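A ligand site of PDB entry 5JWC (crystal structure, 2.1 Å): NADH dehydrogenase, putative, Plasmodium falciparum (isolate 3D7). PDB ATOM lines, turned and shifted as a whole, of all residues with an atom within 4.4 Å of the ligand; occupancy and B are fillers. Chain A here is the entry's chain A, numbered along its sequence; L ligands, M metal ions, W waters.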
ATOM      1  N   LEU A  34      -6.645 -33.995   5.033  1.00  0.00           N
ATOM      2  CA  LEU A  34      -6.281 -34.350   3.677  1.00  0.00           C
ATOM      3  C   LEU A  34      -6.681 -33.218   2.750  1.00  0.00           C
ATOM      4  O   LEU A  34      -7.874 -32.925   2.621  1.00  0.00           O
ATOM      5  CB  LEU A  34      -6.962 -35.635   3.232  1.00  0.00           C
ATOM      6  CG  LEU A  34      -6.712 -36.876   4.077  1.00  0.00           C
ATOM      7  CD1 LEU A  34      -7.387 -38.085   3.406  1.00  0.00           C
ATOM      8  CD2 LEU A  34      -5.199 -37.087   4.267  1.00  0.00           C
ATOM      9  N   GLY A  35      -5.705 -32.594   2.110  1.00  0.00           N
ATOM     10  CA  GLY A  35      -5.985 -31.539   1.137  1.00  0.00           C
ATOM     11  C   GLY A  35      -5.495 -30.189   1.637  1.00  0.00           C
ATOM     12  O   GLY A  35      -5.668 -29.843   2.821  1.00  0.00           O
ATOM     13  N   SER A  36      -4.884 -29.440   0.729  1.00  0.00           N
ATOM     14  CA  SER A  36      -4.396 -28.104   1.048  1.00  0.00           C
ATOM     15  C   SER A  36      -5.205 -27.035   0.299  1.00  0.00           C
ATOM     16  O   SER A  36      -4.661 -26.030  -0.159  1.00  0.00           O
ATOM     17  CB  SER A  36      -2.899 -27.982   0.708  1.00  0.00           C
ATOM     18  OG  SER A  36      -2.624 -28.450  -0.617  1.00  0.00           O
ATOM     19  N   GLY A  37      -6.511 -27.252   0.164  1.00  0.00           N
ATOM     20  CA  GLY A  37      -7.336 -26.360  -0.614  1.00  0.00           C
ATOM     21  C   GLY A  37      -8.212 -25.495   0.267  1.00  0.00           C
ATOM     22  O   GLY A  37      -7.891 -25.260   1.419  1.00  0.00           O
ATOM     23  N   TRP A  38      -9.348 -25.045  -0.267  1.00  0.00           N
ATOM     24  CA  TRP A  38     -10.200 -24.129   0.492  1.00  0.00           C
ATOM     25  C   TRP A  38     -10.645 -24.737   1.813  1.00  0.00           C
ATOM     26  O   TRP A  38     -10.632 -24.071   2.838  1.00  0.00           O
ATOM     27  CB  TRP A  38     -11.404 -23.683  -0.347  1.00  0.00           C
ATOM     28  CG  TRP A  38     -11.045 -22.543  -1.288  1.00  0.00           C
ATOM     29  CD1 TRP A  38     -10.709 -22.635  -2.592  1.00  0.00           C
ATOM     30  CD2 TRP A  38     -10.954 -21.149  -0.944  1.00  0.00           C
ATOM     31  NE1 TRP A  38     -10.422 -21.395  -3.109  1.00  0.00           N
ATOM     32  CE2 TRP A  38     -10.561 -20.459  -2.122  1.00  0.00           C
ATOM     33  CE3 TRP A  38     -11.168 -20.408   0.223  1.00  0.00           C
ATOM     34  CZ2 TRP A  38     -10.399 -19.076  -2.155  1.00  0.00           C
ATOM     35  CZ3 TRP A  38     -10.995 -19.035   0.190  1.00  0.00           C
ATOM     36  CH2 TRP A  38     -10.608 -18.381  -0.985  1.00  0.00           C
ATOM     37  N   GLY A  39     -11.010 -26.002   1.812  1.00  0.00           N
ATOM     38  CA  GLY A  39     -11.389 -26.649   3.044  1.00  0.00           C
ATOM     39  C   GLY A  39     -10.195 -26.917   3.949  1.00  0.00           C
ATOM     40  O   GLY A  39     -10.151 -26.468   5.108  1.00  0.00           O
ATOM     41  N   GLY A  40      -9.219 -27.665   3.425  1.00  0.00           N
ATOM     42  CA  GLY A  40      -8.092 -28.116   4.212  1.00  0.00           C
ATOM     43  C   GLY A  40      -7.290 -26.967   4.802  1.00  0.00           C
ATOM     44  O   GLY A  40      -7.014 -26.962   6.006  1.00  0.00           O
ATOM     45  N   ILE A  57      -1.866 -33.198   5.005  1.00  0.00           N
ATOM     46  CA  ILE A  57      -1.304 -34.055   3.991  1.00  0.00           C
ATOM     47  C   ILE A  57      -1.909 -33.721   2.639  1.00  0.00           C
ATOM     48  O   ILE A  57      -3.124 -33.784   2.457  1.00  0.00           O
ATOM     49  CB  ILE A  57      -1.562 -35.531   4.334  1.00  0.00           C
ATOM     50  CG1 ILE A  57      -0.877 -35.862   5.652  1.00  0.00           C
ATOM     51  CG2 ILE A  57      -1.021 -36.407   3.263  1.00  0.00           C
ATOM     52  CD1 ILE A  57      -1.191 -37.229   6.150  1.00  0.00           C
ATOM     53  N   SER A  58      -1.063 -33.378   1.676  1.00  0.00           N
ATOM     54  CA  SER A  58      -1.506 -33.041   0.329  1.00  0.00           C
ATOM     55  C   SER A  58      -0.334 -33.122  -0.631  1.00  0.00           C
ATOM     56  O   SER A  58       0.786 -32.814  -0.241  1.00  0.00           O
ATOM     57  CB  SER A  58      -2.108 -31.631   0.304  1.00  0.00           C
ATOM     58  OG  SER A  58      -2.420 -31.261  -1.012  1.00  0.00           O
ATOM     59  N   PRO A  59      -0.583 -33.532  -1.891  1.00  0.00           N
ATOM     60  CA  PRO A  59       0.538 -33.546  -2.840  1.00  0.00           C
ATOM     61  C   PRO A  59       0.928 -32.133  -3.277  1.00  0.00           C
ATOM     62  O   PRO A  59       1.959 -31.949  -3.917  1.00  0.00           O
ATOM     63  CB  PRO A  59      -0.002 -34.359  -4.023  1.00  0.00           C
ATOM     64  CG  PRO A  59      -1.502 -34.146  -3.960  1.00  0.00           C
ATOM     65  CD  PRO A  59      -1.825 -34.059  -2.481  1.00  0.00           C
ATOM     66  N   ARG A  60       0.103 -31.153  -2.901  1.00  0.00           N
ATOM     67  CA  ARG A  60       0.316 -29.753  -3.257  1.00  0.00           C
ATOM     68  C   ARG A  60       0.739 -28.981  -2.016  1.00  0.00           C
ATOM     69  O   ARG A  60      -0.024 -28.896  -1.043  1.00  0.00           O
ATOM     70  CB  ARG A  60      -0.986 -29.156  -3.829  1.00  0.00           C
ATOM     71  CG  ARG A  60      -0.826 -27.910  -4.686  1.00  0.00           C
ATOM     72  CD  ARG A  60      -2.208 -27.438  -5.202  1.00  0.00           C
ATOM     73  NE  ARG A  60      -3.028 -26.911  -4.119  1.00  0.00           N
ATOM     74  CZ  ARG A  60      -4.303 -26.570  -4.249  1.00  0.00           C
ATOM     75  NH1 ARG A  60      -4.907 -26.690  -5.424  1.00  0.00           N
ATOM     76  NH2 ARG A  60      -4.969 -26.095  -3.206  1.00  0.00           N
ATOM     77  N   THR A  66      -8.351 -20.106  -5.922  1.00  0.00           N
ATOM     78  CA  THR A  66      -8.969 -20.438  -7.218  1.00  0.00           C
ATOM     79  C   THR A  66      -9.783 -19.324  -7.921  1.00  0.00           C
ATOM     80  O   THR A  66      -9.770 -19.256  -9.144  1.00  0.00           O
ATOM     81  CB  THR A  66      -9.889 -21.670  -7.085  1.00  0.00           C
ATOM     82  OG1 THR A  66     -10.784 -21.483  -5.984  1.00  0.00           O
ATOM     83  CG2 THR A  66      -9.054 -22.924  -6.802  1.00  0.00           C
ATOM     84  N   PRO A  67     -10.502 -18.466  -7.153  1.00  0.00           N
ATOM     85  CA  PRO A  67     -11.280 -17.476  -7.917  1.00  0.00           C
ATOM     86  C   PRO A  67     -10.470 -16.542  -8.840  1.00  0.00           C
ATOM     87  O   PRO A  67     -11.052 -15.943  -9.745  1.00  0.00           O
ATOM     88  CB  PRO A  67     -11.952 -16.634  -6.828  1.00  0.00           C
ATOM     89  CG  PRO A  67     -12.049 -17.547  -5.653  1.00  0.00           C
ATOM     90  CD  PRO A  67     -10.780 -18.382  -5.704  1.00  0.00           C
ATOM     91  N   LEU A  69      -7.798 -17.467 -10.681  1.00  0.00           N
ATOM     92  CA  LEU A  69      -7.127 -18.252 -11.727  1.00  0.00           C
ATOM     93  C   LEU A  69      -7.344 -17.699 -13.171  1.00  0.00           C
ATOM     94  O   LEU A  69      -6.404 -17.692 -13.973  1.00  0.00           O
ATOM     95  CB  LEU A  69      -7.609 -19.702 -11.649  1.00  0.00           C
ATOM     96  CG  LEU A  69      -6.860 -20.562 -10.607  1.00  0.00           C
ATOM     97  CD1 LEU A  69      -7.397 -21.974 -10.597  1.00  0.00           C
ATOM     98  CD2 LEU A  69      -5.353 -20.586 -10.850  1.00  0.00           C
ATOM     99  N   LEU A 103       2.364 -35.658   0.517  1.00  0.00           N
ATOM    100  CA  LEU A 103       1.990 -37.018   0.179  1.00  0.00           C
ATOM    101  C   LEU A 103       0.604 -36.992  -0.455  1.00  0.00           C
ATOM    102  O   LEU A 103      -0.191 -36.097  -0.172  1.00  0.00           O
ATOM    103  CB  LEU A 103       1.975 -37.891   1.427  1.00  0.00           C
ATOM    104  CG  LEU A 103       3.276 -38.093   2.197  1.00  0.00           C
ATOM    105  CD1 LEU A 103       2.970 -38.731   3.542  1.00  0.00           C
ATOM    106  CD2 LEU A 103       4.222 -38.970   1.379  1.00  0.00           C
ATOM    107  N   GLU A 104       0.330 -37.994  -1.281  1.00  0.00           N
ATOM    108  CA  GLU A 104      -0.996 -38.245  -1.813  1.00  0.00           C
ATOM    109  C   GLU A 104      -1.638 -39.414  -1.058  1.00  0.00           C
ATOM    110  O   GLU A 104      -1.045 -40.501  -0.988  1.00  0.00           O
ATOM    111  CB  GLU A 104      -0.914 -38.548  -3.313  1.00  0.00           C
ATOM    112  CG  GLU A 104      -2.218 -39.006  -3.920  1.00  0.00           C
ATOM    113  CD  GLU A 104      -2.049 -39.589  -5.307  1.00  0.00           C
ATOM    114  OE1 GLU A 104      -1.144 -39.144  -6.052  1.00  0.00           O
ATOM    115  OE2 GLU A 104      -2.830 -40.495  -5.658  1.00  0.00           O
ATOM    116  N   CYS A 105      -2.822 -39.215  -0.483  1.00  0.00           N
ATOM    117  CA  CYS A 105      -3.528 -40.313   0.181  1.00  0.00           C
ATOM    118  C   CYS A 105      -4.181 -41.250  -0.840  1.00  0.00           C
ATOM    119  O   CYS A 105      -4.807 -40.794  -1.804  1.00  0.00           O
ATOM    120  CB  CYS A 105      -4.570 -39.795   1.166  1.00  0.00           C
ATOM    121  SG  CYS A 105      -5.395 -41.110   2.112  1.00  0.00           S
ATOM    122  N   ALA A 135     -10.700 -33.451   2.838  1.00  0.00           N
ATOM    123  CA  ALA A 135     -10.963 -32.246   2.066  1.00  0.00           C
ATOM    124  C   ALA A 135     -10.191 -32.296   0.747  1.00  0.00           C
ATOM    125  O   ALA A 135      -9.467 -31.347   0.418  1.00  0.00           O
ATOM    126  CB  ALA A 135     -10.568 -31.007   2.866  1.00  0.00           C
ATOM    127  N   VAL A 136     -10.355 -33.382   0.003  1.00  0.00           N
ATOM    128  CA  VAL A 136      -9.545 -33.632  -1.196  1.00  0.00           C
ATOM    129  C   VAL A 136     -10.128 -33.038  -2.460  1.00  0.00           C
ATOM    130  O   VAL A 136      -9.583 -33.208  -3.557  1.00  0.00           O
ATOM    131  CB  VAL A 136      -9.325 -35.128  -1.423  1.00  0.00           C
ATOM    132  CG1 VAL A 136      -8.568 -35.714  -0.231  1.00  0.00           C
ATOM    133  CG2 VAL A 136     -10.690 -35.859  -1.639  1.00  0.00           C
ATOM    134  N   GLY A 137     -11.250 -32.339  -2.326  1.00  0.00           N
ATOM    135  CA  GLY A 137     -11.847 -31.684  -3.466  1.00  0.00           C
ATOM    136  C   GLY A 137     -12.337 -32.643  -4.543  1.00  0.00           C
ATOM    137  O   GLY A 137     -12.821 -33.730  -4.247  1.00  0.00           O
ATOM    138  N   VAL A 155      -8.856 -25.810 -16.549  1.00  0.00           N
ATOM    139  CA  VAL A 155      -8.614 -24.615 -15.759  1.00  0.00           C
ATOM    140  C   VAL A 155      -8.888 -24.882 -14.298  1.00  0.00           C
ATOM    141  O   VAL A 155      -9.841 -24.334 -13.747  1.00  0.00           O
ATOM    142  CB  VAL A 155      -9.497 -23.404 -16.172  1.00  0.00           C
ATOM    143  CG1 VAL A 155      -8.868 -22.092 -15.701  1.00  0.00           C
ATOM    144  CG2 VAL A 155      -9.695 -23.378 -17.630  1.00  0.00           C
ATOM    145  N   LYS A 156      -8.098 -25.722 -13.657  1.00  0.00           N
ATOM    146  CA  LYS A 156      -8.451 -26.056 -12.283  1.00  0.00           C
ATOM    147  C   LYS A 156      -7.408 -25.621 -11.271  1.00  0.00           C
ATOM    148  O   LYS A 156      -7.724 -25.442 -10.096  1.00  0.00           O
ATOM    149  CB  LYS A 156      -8.729 -27.553 -12.157  1.00  0.00           C
ATOM    150  CG  LYS A 156     -10.170 -27.836 -11.678  1.00  0.00           C
ATOM    151  CD  LYS A 156     -10.252 -29.149 -10.943  1.00  0.00           C
ATOM    152  CE  LYS A 156      -9.489 -29.014  -9.647  1.00  0.00           C
ATOM    153  NZ  LYS A 156     -10.062 -29.753  -8.544  1.00  0.00           N
ATOM    154  N   THR A 199     -16.275 -19.372 -14.567  1.00  0.00           N
ATOM    155  CA  THR A 199     -14.899 -19.583 -15.008  1.00  0.00           C
ATOM    156  C   THR A 199     -14.712 -19.384 -16.510  1.00  0.00           C
ATOM    157  O   THR A 199     -13.839 -18.612 -16.924  1.00  0.00           O
ATOM    158  CB  THR A 199     -14.403 -20.965 -14.649  1.00  0.00           C
ATOM    159  OG1 THR A 199     -14.384 -21.082 -13.227  1.00  0.00           O
ATOM    160  CG2 THR A 199     -12.985 -21.159 -15.184  1.00  0.00           C
ATOM    161  N   LEU A 304      -9.389 -41.424  -4.754  1.00  0.00           N
ATOM    162  CA  LEU A 304      -9.413 -41.726  -3.327  1.00  0.00           C
ATOM    163  C   LEU A 304     -10.836 -41.873  -2.780  1.00  0.00           C
ATOM    164  O   LEU A 304     -11.142 -42.798  -2.018  1.00  0.00           O
ATOM    165  CB  LEU A 304      -8.686 -40.633  -2.545  1.00  0.00           C
ATOM    166  CG  LEU A 304      -8.873 -40.670  -1.031  1.00  0.00           C
ATOM    167  CD1 LEU A 304      -8.331 -41.994  -0.484  1.00  0.00           C
ATOM    168  CD2 LEU A 304      -8.224 -39.510  -0.336  1.00  0.00           C
ATOM    169  N   ILE A 340     -15.306 -32.216   4.194  1.00  0.00           N
ATOM    170  CA  ILE A 340     -15.767 -30.853   3.928  1.00  0.00           C
ATOM    171  C   ILE A 340     -15.447 -30.470   2.489  1.00  0.00           C
ATOM    172  O   ILE A 340     -14.581 -31.093   1.868  1.00  0.00           O
ATOM    173  CB  ILE A 340     -15.116 -29.824   4.873  1.00  0.00           C
ATOM    174  CG1 ILE A 340     -13.592 -29.803   4.676  1.00  0.00           C
ATOM    175  CG2 ILE A 340     -15.436 -30.128   6.329  1.00  0.00           C
ATOM    176  CD1 ILE A 340     -12.877 -28.821   5.664  1.00  0.00           C
ATOM    177  N   GLY A 341     -16.125 -29.458   1.957  1.00  0.00           N
ATOM    178  CA  GLY A 341     -15.802 -29.005   0.606  1.00  0.00           C
ATOM    179  C   GLY A 341     -16.440 -29.820  -0.501  1.00  0.00           C
ATOM    180  O   GLY A 341     -17.486 -30.445  -0.313  1.00  0.00           O
ATOM    181  N   ASP A 342     -15.808 -29.807  -1.681  1.00  0.00           N
ATOM    182  CA  ASP A 342     -16.384 -30.382  -2.902  1.00  0.00           C
ATOM    183  C   ASP A 342     -16.471 -31.919  -2.928  1.00  0.00           C
ATOM    184  O   ASP A 342     -17.128 -32.481  -3.800  1.00  0.00           O
ATOM    185  CB  ASP A 342     -15.568 -29.976  -4.117  1.00  0.00           C
ATOM    186  CG  ASP A 342     -15.767 -28.521  -4.516  1.00  0.00           C
ATOM    187  OD1 ASP A 342     -16.506 -27.780  -3.833  1.00  0.00           O
ATOM    188  OD2 ASP A 342     -15.130 -28.127  -5.515  1.00  0.00           O
ATOM    189  N   PRO A 422     -20.952 -26.600  -4.337  1.00  0.00           N
ATOM    190  CA  PRO A 422     -19.492 -26.806  -4.330  1.00  0.00           C
ATOM    191  C   PRO A 422     -18.726 -25.511  -4.626  1.00  0.00           C
ATOM    192  O   PRO A 422     -18.289 -25.284  -5.760  1.00  0.00           O
ATOM    193  CB  PRO A 422     -19.263 -27.838  -5.423  1.00  0.00           C
ATOM    194  CG  PRO A 422     -20.398 -27.578  -6.415  1.00  0.00           C
ATOM    195  CD  PRO A 422     -21.586 -27.174  -5.548  1.00  0.00           C
ATOM    196  N   THR A 423     -18.571 -24.669  -3.611  1.00  0.00           N
ATOM    197  CA  THR A 423     -17.890 -23.387  -3.758  1.00  0.00           C
ATOM    198  C   THR A 423     -16.796 -23.164  -2.712  1.00  0.00           C
ATOM    199  O   THR A 423     -16.780 -23.824  -1.667  1.00  0.00           O
ATOM    200  CB  THR A 423     -18.876 -22.224  -3.656  1.00  0.00           C
ATOM    201  OG1 THR A 423     -19.454 -22.218  -2.341  1.00  0.00           O
ATOM    202  CG2 THR A 423     -20.000 -22.355  -4.716  1.00  0.00           C
ATOM    203  N   ALA A 424     -15.893 -22.236  -3.004  1.00  0.00           N
ATOM    204  CA  ALA A 424     -14.870 -21.870  -2.038  1.00  0.00           C
ATOM    205  C   ALA A 424     -15.526 -21.262  -0.808  1.00  0.00           C
ATOM    206  O   ALA A 424     -15.087 -21.512   0.312  1.00  0.00           O
ATOM    207  CB  ALA A 424     -13.860 -20.898  -2.649  1.00  0.00           C
ATOM    208  N   GLN A 425     -16.577 -20.485  -1.029  1.00  0.00           N
ATOM    209  CA  GLN A 425     -17.321 -19.879   0.071  1.00  0.00           C
ATOM    210  C   GLN A 425     -17.796 -20.938   1.050  1.00  0.00           C
ATOM    211  O   GLN A 425     -17.606 -20.818   2.250  1.00  0.00           O
ATOM    212  CB  GLN A 425     -18.523 -19.073  -0.428  1.00  0.00           C
ATOM    213  CG  GLN A 425     -18.156 -17.773  -1.120  1.00  0.00           C
ATOM    214  CD  GLN A 425     -19.358 -17.063  -1.720  1.00  0.00           C
ATOM    215  OE1 GLN A 425     -20.340 -17.708  -2.101  1.00  0.00           O
ATOM    216  NE2 GLN A 425     -19.298 -15.742  -1.809  1.00  0.00           N
ATOM    217  N   ALA A 427     -16.757 -24.189   1.284  1.00  0.00           N
ATOM    218  CA  ALA A 427     -15.624 -24.928   1.860  1.00  0.00           C
ATOM    219  C   ALA A 427     -14.993 -24.132   3.004  1.00  0.00           C
ATOM    220  O   ALA A 427     -14.637 -24.696   4.040  1.00  0.00           O
ATOM    221  CB  ALA A 427     -14.577 -25.265   0.777  1.00  0.00           C
ATOM    222  N   TYR A 492     -12.235  -8.442  -3.339  1.00  0.00           N
ATOM    223  CA  TYR A 492     -11.188  -9.456  -3.345  1.00  0.00           C
ATOM    224  C   TYR A 492     -10.008  -9.170  -2.434  1.00  0.00           C
ATOM    225  O   TYR A 492      -9.446 -10.109  -1.868  1.00  0.00           O
ATOM    226  CB  TYR A 492     -10.692  -9.713  -4.783  1.00  0.00           C
ATOM    227  CG  TYR A 492     -11.528 -10.796  -5.379  1.00  0.00           C
ATOM    228  CD1 TYR A 492     -11.501 -12.069  -4.840  1.00  0.00           C
ATOM    229  CD2 TYR A 492     -12.415 -10.553  -6.421  1.00  0.00           C
ATOM    230  CE1 TYR A 492     -12.284 -13.092  -5.342  1.00  0.00           C
ATOM    231  CE2 TYR A 492     -13.213 -11.570  -6.938  1.00  0.00           C
ATOM    232  CZ  TYR A 492     -13.146 -12.833  -6.388  1.00  0.00           C
ATOM    233  OH  TYR A 492     -13.929 -13.856  -6.890  1.00  0.00           O
HETATM  234  P1  LIG L   1      -9.756 -27.772  -3.369  1.00  0.00           P
HETATM  235  O1  LIG L   1      -9.641 -28.043  -4.836  1.00  0.00           O
HETATM  236  O2  LIG L   1      -9.708 -26.321  -3.013  1.00  0.00           O
HETATM  237  O3  LIG L   1      -8.617 -28.566  -2.562  1.00  0.00           O
HETATM  238  C1  LIG L   1      -8.455 -29.966  -2.679  1.00  0.00           C
HETATM  239  C2  LIG L   1      -7.073 -30.286  -2.130  1.00  0.00           C
HETATM  240  O4  LIG L   1      -6.948 -31.684  -1.980  1.00  0.00           O
HETATM  241  C3  LIG L   1      -5.974 -29.835  -3.099  1.00  0.00           C
HETATM  242  O5  LIG L   1      -4.911 -29.297  -2.342  1.00  0.00           O
HETATM  243  C4  LIG L   1      -5.495 -31.129  -3.710  1.00  0.00           C
HETATM  244  O6  LIG L   1      -4.128 -31.049  -4.061  1.00  0.00           O
HETATM  245  C5  LIG L   1      -5.715 -32.077  -2.537  1.00  0.00           C
HETATM  246  N1  LIG L   1      -5.811 -33.497  -2.875  1.00  0.00           N
HETATM  247  C6  LIG L   1      -6.373 -34.062  -3.997  1.00  0.00           C
HETATM  248  N2  LIG L   1      -6.264 -35.404  -3.875  1.00  0.00           N
HETATM  249  C7  LIG L   1      -5.639 -35.699  -2.714  1.00  0.00           C
HETATM  250  C8  LIG L   1      -5.286 -36.903  -2.131  1.00  0.00           C
HETATM  251  N3  LIG L   1      -5.628 -38.058  -2.702  1.00  0.00           N
HETATM  252  N4  LIG L   1      -4.660 -36.885  -0.901  1.00  0.00           N
HETATM  253  C9  LIG L   1      -4.394 -35.689  -0.271  1.00  0.00           C
HETATM  254  N5  LIG L   1      -4.752 -34.489  -0.870  1.00  0.00           N
HETATM  255  C10 LIG L   1      -5.355 -34.505  -2.076  1.00  0.00           C
HETATM  256  N6  LIG L   1     -15.812 -20.829  -5.595  1.00  0.00           N
HETATM  257  C11 LIG L   1     -16.409 -19.701  -5.105  1.00  0.00           C
HETATM  258  O7  LIG L   1     -17.069 -19.766  -4.077  1.00  0.00           O
HETATM  259  N7  LIG L   1     -16.266 -18.481  -5.750  1.00  0.00           N
HETATM  260  C12 LIG L   1     -15.520 -18.363  -6.893  1.00  0.00           C
HETATM  261  O8  LIG L   1     -15.397 -17.260  -7.439  1.00  0.00           O
HETATM  262  C13 LIG L   1     -14.890 -19.498  -7.384  1.00  0.00           C
HETATM  263  N8  LIG L   1     -14.125 -19.431  -8.533  1.00  0.00           N
HETATM  264  C14 LIG L   1     -13.506 -20.588  -9.004  1.00  0.00           C
HETATM  265  C15 LIG L   1     -12.713 -20.524 -10.141  1.00  0.00           C
HETATM  266  C16 LIG L   1     -12.088 -21.654 -10.644  1.00  0.00           C
HETATM  267  C17 LIG L   1     -11.245 -21.533 -11.887  1.00  0.00           C
HETATM  268  C18 LIG L   1     -12.237 -22.869  -9.986  1.00  0.00           C
HETATM  269  C19 LIG L   1     -11.569 -24.106 -10.513  1.00  0.00           C
HETATM  270  C20 LIG L   1     -13.034 -22.938  -8.841  1.00  0.00           C
HETATM  271  C21 LIG L   1     -13.654 -21.803  -8.346  1.00  0.00           C
HETATM  272  N9  LIG L   1     -14.439 -21.860  -7.201  1.00  0.00           N
HETATM  273  C22 LIG L   1     -15.037 -20.722  -6.731  1.00  0.00           C
HETATM  274  C23 LIG L   1     -14.672 -23.154  -6.490  1.00  0.00           C
HETATM  275  C24 LIG L   1     -13.677 -23.511  -5.420  1.00  0.00           C
HETATM  276  O9  LIG L   1     -12.394 -23.518  -5.981  1.00  0.00           O
HETATM  277  C25 LIG L   1     -13.990 -24.927  -4.961  1.00  0.00           C
HETATM  278  O10 LIG L   1     -15.335 -25.037  -4.565  1.00  0.00           O
HETATM  279  C26 LIG L   1     -13.047 -25.219  -3.806  1.00  0.00           C
HETATM  280  O11 LIG L   1     -11.784 -25.398  -4.358  1.00  0.00           O
HETATM  281  C27 LIG L   1     -13.462 -26.440  -3.009  1.00  0.00           C
HETATM  282  O12 LIG L   1     -12.561 -26.560  -1.918  1.00  0.00           O
HETATM  283  P2  LIG L   1     -11.964 -28.002  -1.530  1.00  0.00           P
HETATM  284  O13 LIG L   1     -11.126 -27.859  -0.281  1.00  0.00           O
HETATM  285  O14 LIG L   1     -13.138 -28.938  -1.397  1.00  0.00           O
HETATM  286  O15 LIG L   1     -11.114 -28.459  -2.821  1.00  0.00           O
HETATM  287 MG    MG M   1     -11.381 -29.450  -6.182  1.00  0.00          MG
HETATM  288 MG    MG M   2      -8.849 -28.774   0.771  1.00  0.00          MG
HETATM  289 MG    MG M   3     -13.246 -31.517  -0.587  1.00  0.00          MG
HETATM  290 MG    MG M   4      -7.381 -24.482  -3.493  1.00  0.00          MG
HETATM  291  O   HOH W   1     -17.092 -19.332 -10.078  1.00  0.00           O
HETATM  292  O   HOH W   2     -18.229 -16.586  -4.997  1.00  0.00           O
HETATM  293  O   HOH W   3      -9.056 -26.641  -7.977  1.00  0.00           O
HETATM  294  O   HOH W   4      -7.696 -26.273  -5.719  1.00  0.00           O
HETATM  295  O   HOH W   5     -18.137 -15.185  -7.205  1.00  0.00           O
HETATM  296  O   HOH W   6     -13.487 -26.585  -9.037  1.00  0.00           O
HETATM  297  O   HOH W   7      -7.786 -29.691  -6.308  1.00  0.00           O
HETATM  298  O   HOH W   8     -11.425 -26.165  -7.216  1.00  0.00           O
HETATM  299  O   HOH W   9     -13.862 -15.886  -9.946  1.00  0.00           O
HETATM  300  O   HOH W  10      -3.900 -31.206  -6.594  1.00  0.00           O
HETATM  301  O   HOH W  11      -7.156 -39.437  -5.236  1.00  0.00           O
HETATM  302  O   HOH W  12     -15.114 -18.412 -11.547  1.00  0.00           O
HETATM  303  O   HOH W  13     -16.390 -26.780  -7.376  1.00  0.00           O
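An oxygen (O4) of the ligand lies close to the backbone carbonyl oxygen of Ala 135 (3.5 Å).
The backbone carbonyl oxygen (O) of Val 136 sits close to an oxygen (O4) of the ligand, at 3.4 Å.
CA of Gly 35 touches O4 of the ligand (3.3 Å).
Gly 37 touches the ligand (CA to O3, 3.2 Å).
O of Ile 57 touches C9 of the ligand, 3.6 Å away.
Pro 59 touches the ligand.
Pro 67 touches the ligand.
Glu 104 touches the ligand (CG to N3, 3.7 Å).
Gly 137 touches the ligand.
O of Val 155 touches C17 of the ligand (3.6 Å).
Thr 199 touches the ligand (OG1 to C17, 3.4 Å).
CD2 of Leu 304 touches N3 of the ligand, 3.8 Å away.
Gly 341 touches the ligand (CA to O14, 3.3 Å).
CB of Ala 427 touches O12 of the ligand (3.6 Å).
Tyr 492 touches the ligand (OH to O8, 3.7 Å).
Hydrophobic or aromatic side chains within 4 Å of the ligand: Trp 38, Pro 59, Pro 67, Val 136, Leu 304, Ala 424 and Ala 427.
27 residues have an atom within 4 Å of the ligand: Gly 35, Ser 36, Gly 37, Trp 38, Gly 39, Ile 57, Ser 58, Pro 59, Arg 60, Thr 66, Pro 67, Glu 104, Cys 105, Ala 135, Val 136, Gly 137, Val 155, Thr 199, Leu 304, Gly 341, Asp 342, Pro 422, Thr 423, Ala 424, Gln 425, Ala 427 and Tyr 492.
O9 of the ligand sits at hydrogen-bond distance from OG1 of Thr 66.
An oxygen (O13) of the ligand sits at hydrogen-bond distance from the backbone NH (N) of Gly 39 (2.8 Å).
The backbone NH (N) of Asp 342 sits at hydrogen-bond distance from an oxygen (O14) of the ligand.
The side-chain carboxylate (OD1) of Asp 342 is in hydrogen-bond range of an oxygen (O10) of the ligand (3.1 Å).
N of Ala 424 lies within hydrogen-bond range of O7 of the ligand (2.9 Å).
The backbone NH (N) of Ser 36 lies within hydrogen-bond range of an oxygen (O5) of the ligand (3.1 Å).
An oxygen (O5) of the ligand lies within hydrogen-bond range of the side-chain hydroxyl of Ser 36 (3.0 Å).
The backbone NH (N) of Cys 105 lies within hydrogen-bond range of a nitrogen (N4) of the ligand (3.0 Å).
O of Cys 105 sits at hydrogen-bond distance from N3 of the ligand, at 3.0 Å.
The backbone NH of Thr 423 lies close to an oxygen (O10) of the ligand.
The backbone carbonyl oxygen (O) of Thr 423 lies close to an oxygen (O10) of the ligand.
O2 of the ligand lies within hydrogen-bond range of N of Trp 38 (3.0 Å).
The backbone NH (N) of Gln 425 sits at hydrogen-bond distance from an oxygen (O7) of the ligand (3.2 Å).
The backbone carbonyl oxygen of Pro 422 is in hydrogen-bond range of an oxygen (O10) of the ligand (3.2 Å).
O5 of the ligand is in hydrogen-bond range of NH2 of Arg 60 (3.3 Å).
O5 of the ligand lies within hydrogen-bond range of OG of Ser 58 (3.4 Å).
The indole nitrogen (NE1) of Trp 38 is in hydrogen-bond range of the side-chain hydroxyl (OG1) of Thr 66 (2.9 Å).
OG of Ser 36 is in hydrogen-bond range of O of Arg 60.
OG of Ser 36 sits at hydrogen-bond distance from OG of Ser 58.
The backbone carbonyl oxygen (O) of Ile 57 lies within hydrogen-bond range of the backbone NH (N) of Gly 35, 2.9 Å away.
The backbone NH (N) of Arg 60 sits close to the side-chain hydroxyl (OG) of Ser 58 (3.2 Å).
The backbone NH (N) of Leu 103 sits at hydrogen-bond distance from the backbone carbonyl oxygen (O) of Ser 58 (3.3 Å).
The backbone carbonyl oxygen of Leu 34 lies within hydrogen-bond range of the backbone NH of Ala 135 (2.9 Å).
Water W4 lies within hydrogen-bond range of O1 of the ligand (2.8 Å) and NH1 of Arg 60 (2.8 Å).
Water W7 lies within hydrogen-bond range of O1 of the ligand (2.9 Å) and NZ of Lys 156 (3.2 Å).
Water W9 lies within hydrogen-bond range of the backbone carbonyl oxygen (O) of Pro 67 and an oxygen (O8) of the ligand.
Water W11 lies within hydrogen-bond range of N of Leu 304 (3.0 Å) and N3 of the ligand (3.3 Å).
Water W12 lies within hydrogen-bond range of the side-chain hydroxyl (OG1) of Thr 199 (3.2 Å) and a nitrogen (N8) of the ligand (3.3 Å).
Water W3 lies within hydrogen-bond range of O of Lys 156 (2.8 Å) and O1 of the ligand (3.5 Å).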
